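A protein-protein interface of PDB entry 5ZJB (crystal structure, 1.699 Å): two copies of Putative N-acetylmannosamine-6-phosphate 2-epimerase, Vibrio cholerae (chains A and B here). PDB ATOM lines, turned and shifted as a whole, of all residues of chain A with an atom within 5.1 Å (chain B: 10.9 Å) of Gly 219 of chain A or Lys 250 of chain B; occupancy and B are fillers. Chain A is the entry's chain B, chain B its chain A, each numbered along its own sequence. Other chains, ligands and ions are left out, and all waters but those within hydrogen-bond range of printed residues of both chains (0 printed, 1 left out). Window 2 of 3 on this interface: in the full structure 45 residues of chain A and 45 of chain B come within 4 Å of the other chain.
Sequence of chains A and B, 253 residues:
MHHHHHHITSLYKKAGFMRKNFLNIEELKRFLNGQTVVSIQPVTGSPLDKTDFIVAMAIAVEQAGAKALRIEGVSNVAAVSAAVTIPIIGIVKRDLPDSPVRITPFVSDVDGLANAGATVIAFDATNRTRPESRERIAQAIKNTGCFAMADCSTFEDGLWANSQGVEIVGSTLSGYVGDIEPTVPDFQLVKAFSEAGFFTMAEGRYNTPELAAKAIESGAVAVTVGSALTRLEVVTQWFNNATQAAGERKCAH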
ATOM      1  N   ASN A  33      33.738  -1.411 -21.764  1.00  0.00           N
ATOM      2  CA  ASN A  33      32.883  -1.977 -20.733  1.00  0.00           C
ATOM      3  C   ASN A  33      32.606  -0.956 -19.638  1.00  0.00           C
ATOM      4  O   ASN A  33      33.535  -0.358 -19.083  1.00  0.00           O
ATOM      5  CB  ASN A  33      33.512  -3.225 -20.119  1.00  0.00           C
ATOM      6  CG  ASN A  33      32.549  -3.931 -19.184  1.00  0.00           C
ATOM      7  OD1 ASN A  33      31.528  -4.457 -19.625  1.00  0.00           O
ATOM      8  ND2 ASN A  33      32.843  -3.908 -17.885  1.00  0.00           N
ATOM      9  N   VAL A 190      17.521  -3.844 -24.893  1.00  0.00           N
ATOM     10  CA  VAL A 190      18.902  -3.993 -24.442  1.00  0.00           C
ATOM     11  C   VAL A 190      19.101  -5.349 -23.782  1.00  0.00           C
ATOM     12  O   VAL A 190      20.076  -6.058 -24.064  1.00  0.00           O
ATOM     13  CB  VAL A 190      19.275  -2.846 -23.487  1.00  0.00           C
ATOM     14  CG1 VAL A 190      20.577  -3.150 -22.758  1.00  0.00           C
ATOM     15  CG2 VAL A 190      19.366  -1.546 -24.271  1.00  0.00           C
ATOM     16  N   SER A 194      21.579  -8.299 -25.153  1.00  0.00           N
ATOM     17  CA  SER A 194      22.651  -8.837 -24.321  1.00  0.00           C
ATOM     18  C   SER A 194      22.455 -10.325 -24.068  1.00  0.00           C
ATOM     19  O   SER A 194      23.427 -11.088 -24.088  1.00  0.00           O
ATOM     20  CB  SER A 194      22.751  -8.085 -22.996  1.00  0.00           C
ATOM     21  OG  SER A 194      21.508  -8.033 -22.339  1.00  0.00           O
ATOM     22  N   THR A 200      26.361  -5.220 -27.084  1.00  0.00           N
ATOM     23  CA  THR A 200      25.166  -4.382 -27.043  1.00  0.00           C
ATOM     24  C   THR A 200      25.509  -2.975 -26.576  1.00  0.00           C
ATOM     25  O   THR A 200      26.081  -2.796 -25.499  1.00  0.00           O
ATOM     26  CB  THR A 200      24.104  -4.971 -26.111  1.00  0.00           C
ATOM     27  OG1 THR A 200      23.728  -6.280 -26.577  1.00  0.00           O
ATOM     28  CG2 THR A 200      22.876  -4.086 -26.100  1.00  0.00           C
ATOM     29  N   ALA A 215      20.975   0.620 -17.840  1.00  0.00           N
ATOM     30  CA  ALA A 215      21.297  -0.019 -19.114  1.00  0.00           C
ATOM     31  C   ALA A 215      22.459  -0.987 -18.957  1.00  0.00           C
ATOM     32  O   ALA A 215      22.413  -2.110 -19.480  1.00  0.00           O
ATOM     33  CB  ALA A 215      21.608   1.035 -20.177  1.00  0.00           C
ATOM     34  N   ILE A 216      23.514  -0.569 -18.244  1.00  0.00           N
ATOM     35  CA  ILE A 216      24.656  -1.446 -17.987  1.00  0.00           C
ATOM     36  C   ILE A 216      24.211  -2.677 -17.210  1.00  0.00           C
ATOM     37  O   ILE A 216      24.591  -3.812 -17.531  1.00  0.00           O
ATOM     38  CB  ILE A 216      25.757  -0.689 -17.222  1.00  0.00           C
ATOM     39  CG1 ILE A 216      26.262   0.528 -18.006  1.00  0.00           C
ATOM     40  CG2 ILE A 216      26.905  -1.634 -16.879  1.00  0.00           C
ATOM     41  CD1 ILE A 216      26.870   0.202 -19.352  1.00  0.00           C
ATOM     42  N   GLU A 217      23.429  -2.457 -16.145  1.00  0.00           N
ATOM     43  CA  GLU A 217      22.919  -3.569 -15.343  1.00  0.00           C
ATOM     44  C   GLU A 217      22.072  -4.512 -16.183  1.00  0.00           C
ATOM     45  O   GLU A 217      22.064  -5.728 -15.940  1.00  0.00           O
ATOM     46  CB  GLU A 217      22.108  -3.039 -14.160  1.00  0.00           C
ATOM     47  CG  GLU A 217      22.958  -2.253 -13.196  1.00  0.00           C
ATOM     48  CD  GLU A 217      22.159  -1.570 -12.115  1.00  0.00           C
ATOM     49  OE1 GLU A 217      20.908  -1.520 -12.227  1.00  0.00           O
ATOM     50  OE2 GLU A 217      22.797  -1.085 -11.148  1.00  0.00           O
ATOM     51  N   SER A 218      21.366  -3.978 -17.188  1.00  0.00           N
ATOM     52  CA  SER A 218      20.537  -4.792 -18.076  1.00  0.00           C
ATOM     53  C   SER A 218      21.352  -5.609 -19.073  1.00  0.00           C
ATOM     54  O   SER A 218      20.748  -6.369 -19.840  1.00  0.00           O
ATOM     55  CB  SER A 218      19.548  -3.916 -18.848  1.00  0.00           C
ATOM     56  OG  SER A 218      18.718  -3.170 -17.981  1.00  0.00           O
ATOM     57  N   GLY A 219      22.682  -5.465 -19.097  1.00  0.00           N
ATOM     58  CA  GLY A 219      23.536  -6.248 -19.971  1.00  0.00           C
ATOM     59  C   GLY A 219      24.264  -5.470 -21.048  1.00  0.00           C
ATOM     60  O   GLY A 219      25.033  -6.070 -21.806  1.00  0.00           O
ATOM     61  N   ALA A 220      24.052  -4.163 -21.155  1.00  0.00           N
ATOM     62  CA  ALA A 220      24.762  -3.396 -22.166  1.00  0.00           C
ATOM     63  C   ALA A 220      26.257  -3.359 -21.853  1.00  0.00           C
ATOM     64  O   ALA A 220      26.658  -3.245 -20.690  1.00  0.00           O
ATOM     65  CB  ALA A 220      24.184  -1.978 -22.239  1.00  0.00           C
ATOM     66  N   VAL A 221      27.084  -3.480 -22.898  1.00  0.00           N
ATOM     67  CA  VAL A 221      28.516  -3.218 -22.753  1.00  0.00           C
ATOM     68  C   VAL A 221      28.733  -1.766 -22.369  1.00  0.00           C
ATOM     69  O   VAL A 221      29.472  -1.451 -21.430  1.00  0.00           O
ATOM     70  CB  VAL A 221      29.273  -3.558 -24.051  1.00  0.00           C
ATOM     71  CG1 VAL A 221      30.720  -3.126 -23.939  1.00  0.00           C
ATOM     72  CG2 VAL A 221      29.193  -5.049 -24.336  1.00  0.00           C
ATOM     73  N   ALA B 242      28.371   6.607 -12.619  1.00  0.00           N
ATOM     74  CA  ALA B 242      27.259   5.672 -12.488  1.00  0.00           C
ATOM     75  C   ALA B 242      27.474   4.430 -13.352  1.00  0.00           C
ATOM     76  O   ALA B 242      27.264   3.299 -12.889  1.00  0.00           O
ATOM     77  CB  ALA B 242      25.949   6.369 -12.854  1.00  0.00           C
ATOM     78  N   THR B 243      27.880   4.608 -14.613  1.00  0.00           N
ATOM     79  CA  THR B 243      27.964   3.437 -15.494  1.00  0.00           C
ATOM     80  C   THR B 243      29.159   2.566 -15.140  1.00  0.00           C
ATOM     81  O   THR B 243      29.068   1.331 -15.185  1.00  0.00           O
ATOM     82  CB  THR B 243      28.027   3.840 -16.982  1.00  0.00           C
ATOM     83  OG1 THR B 243      29.189   4.651 -17.254  1.00  0.00           O
ATOM     84  CG2 THR B 243      26.736   4.560 -17.419  1.00  0.00           C
ATOM     85  N   GLN B 244      30.285   3.183 -14.791  1.00  0.00           N
ATOM     86  CA  GLN B 244      31.468   2.400 -14.449  1.00  0.00           C
ATOM     87  C   GLN B 244      31.259   1.620 -13.161  1.00  0.00           C
ATOM     88  O   GLN B 244      31.777   0.508 -13.024  1.00  0.00           O
ATOM     89  CB  GLN B 244      32.693   3.309 -14.344  1.00  0.00           C
ATOM     90  CG  GLN B 244      33.184   3.813 -15.697  1.00  0.00           C
ATOM     91  CD  GLN B 244      34.201   4.919 -15.584  1.00  0.00           C
ATOM     92  OE1 GLN B 244      34.635   5.278 -14.485  1.00  0.00           O
ATOM     93  NE2 GLN B 244      34.573   5.494 -16.723  1.00  0.00           N
ATOM     94  N   ALA B 245      30.491   2.170 -12.218  1.00  0.00           N
ATOM     95  CA  ALA B 245      30.145   1.412 -11.019  1.00  0.00           C
ATOM     96  C   ALA B 245      29.229   0.243 -11.354  1.00  0.00           C
ATOM     97  O   ALA B 245      29.385  -0.853 -10.802  1.00  0.00           O
ATOM     98  CB  ALA B 245      29.485   2.323  -9.987  1.00  0.00           C
ATOM     99  N   ALA B 246      28.266   0.457 -12.253  1.00  0.00           N
ATOM    100  CA  ALA B 246      27.395  -0.641 -12.661  1.00  0.00           C
ATOM    101  C   ALA B 246      28.184  -1.730 -13.373  1.00  0.00           C
ATOM    102  O   ALA B 246      27.892  -2.920 -13.212  1.00  0.00           O
ATOM    103  CB  ALA B 246      26.263  -0.128 -13.551  1.00  0.00           C
ATOM    104  N   GLY B 247      29.181  -1.346 -14.176  1.00  0.00           N
ATOM    105  CA  GLY B 247      30.008  -2.343 -14.835  1.00  0.00           C
ATOM    106  C   GLY B 247      30.880  -3.106 -13.861  1.00  0.00           C
ATOM    107  O   GLY B 247      31.175  -4.286 -14.075  1.00  0.00           O
ATOM    108  N   GLU B 248      31.304  -2.446 -12.784  1.00  0.00           N
ATOM    109  CA  GLU B 248      32.039  -3.122 -11.723  1.00  0.00           C
ATOM    110  C   GLU B 248      31.131  -4.074 -10.949  1.00  0.00           C
ATOM    111  O   GLU B 248      31.495  -5.229 -10.700  1.00  0.00           O
ATOM    112  CB  GLU B 248      32.661  -2.075 -10.799  1.00  0.00           C
ATOM    113  CG  GLU B 248      33.500  -2.614  -9.662  1.00  0.00           C
ATOM    114  CD  GLU B 248      34.005  -1.501  -8.758  1.00  0.00           C
ATOM    115  OE1 GLU B 248      33.678  -0.322  -9.024  1.00  0.00           O
ATOM    116  OE2 GLU B 248      34.727  -1.800  -7.783  1.00  0.00           O
ATOM    117  N   ARG B 249      29.936  -3.607 -10.566  1.00  0.00           N
ATOM    118  CA  ARG B 249      28.979  -4.481  -9.889  1.00  0.00           C
ATOM    119  C   ARG B 249      28.697  -5.728 -10.716  1.00  0.00           C
ATOM    120  O   ARG B 249      28.772  -6.856 -10.213  1.00  0.00           O
ATOM    121  CB  ARG B 249      27.675  -3.731  -9.606  1.00  0.00           C
ATOM    122  CG  ARG B 249      27.743  -2.748  -8.456  1.00  0.00           C
ATOM    123  CD  ARG B 249      26.346  -2.371  -7.968  1.00  0.00           C
ATOM    124  NE  ARG B 249      25.537  -1.723  -9.001  1.00  0.00           N
ATOM    125  CZ  ARG B 249      25.679  -0.453  -9.370  1.00  0.00           C
ATOM    126  NH1 ARG B 249      26.611   0.301  -8.803  1.00  0.00           N
ATOM    127  NH2 ARG B 249      24.897   0.063 -10.310  1.00  0.00           N
ATOM    128  N   LYS B 250      28.353  -5.540 -11.992  1.00  0.00           N
ATOM    129  CA  LYS B 250      28.113  -6.673 -12.876  1.00  0.00           C
ATOM    130  C   LYS B 250      29.284  -7.644 -12.856  1.00  0.00           C
ATOM    131  O   LYS B 250      29.092  -8.865 -12.796  1.00  0.00           O
ATOM    132  CB  LYS B 250      27.855  -6.177 -14.300  1.00  0.00           C
ATOM    133  CG  LYS B 250      27.593  -7.283 -15.311  1.00  0.00           C
ATOM    134  CD  LYS B 250      27.769  -6.780 -16.737  1.00  0.00           C
ATOM    135  CE  LYS B 250      26.937  -5.535 -16.991  1.00  0.00           C
ATOM    136  NZ  LYS B 250      26.952  -5.096 -18.417  1.00  0.00           N
ATOM    137  N   CYS B 251      30.505  -7.121 -12.909  1.00  0.00           N
ATOM    138  CA  CYS B 251      31.705  -7.949 -12.881  1.00  0.00           C
ATOM    139  C   CYS B 251      31.781  -8.776 -11.600  1.00  0.00           C
ATOM    140  O   CYS B 251      32.243  -8.298 -10.563  1.00  0.00           O
ATOM    141  CB  CYS B 251      32.952  -7.077 -13.021  1.00  0.00           C
ATOM    142  SG  CYS B 251      34.494  -7.914 -12.608  1.00  0.00           S
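Ser 194 of chain A touches none of the printed residues of chain B. No residue of chain B comes within 4 Å of Thr 200 of chain A. Printed residues of chain B within 4 Å of Glu 217 of chain A: Ala 246 (3.9 Å) and Arg 249 (2.5 Å). No residue of chain B comes within 4 Å of Ser 218 of chain A. Gly 219 of chain A touches just one residue of chain B: Lys 250 (3.8 Å). Ala 220 of chain A touches just one residue of chain B: Lys 250 (2.9 Å). Printed residues of chain A within 4 Å of Thr 243 of chain B: Ile 216 (3.9 Å). Lys 250 of chain B touches three residues of chain A. The nearest printed residue of chain A that does not touch Lys 250 of chain B is Glu 217 of chain A (4.7 Å).
The guanidinium group of Arg 249 of chain B is in salt-bridge range of the side-chain carboxylate of Glu 217 of chain A (2.5 Å). The side-chain amino group (NZ) of Lys 250 of chain B lies within hydrogen-bond range of the backbone carbonyl oxygen (O) of Ile 216 of chain A, 2.8 Å away. The backbone carbonyl oxygen of Ala 220 of chain A sits at hydrogen-bond distance from the side-chain amino group of Lys 250 of chain B, 2.9 Å away.
Among the printed residues, pairs that only touch across the chains: Ile 216 of chain A with Thr 243 of chain B (3.9 Å), Ile 216 of chain A with Ala 246 of chain B (3.7 Å), Ile 216 of chain A with Gly 247 of chain B (3.5 Å), Glu 217 of chain A with Ala 246 of chain B (3.9 Å) and Gly 219 of chain A with Lys 250 of chain B (3.8 Å).
The backbone carbonyl oxygen (O) of Ala 215 of chain A lies within hydrogen-bond range of the backbone NH (N) of Ala 220 of chain A (3.1 Å).
No position is printed for both chains. Of the 8 pairs that touch across the chains among the printed residues, none has its exchanged pair printed and touching as well.
Hydrophobic or aromatic side chains of chain A that line the printed part of chain B: Ile 216. Of the 10 printed residues of chain B, 5 touch a printed residue of chain A. Printed residues of chain B that touch a printed residue of chain A: Thr 243, Ala 246, Gly 247, Arg 249 and Lys 250. Hydrophobic or aromatic side chains of chain B that line the printed part of chain A: Ala 246. Among the printed residues, 8 pairs touch across the chains.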
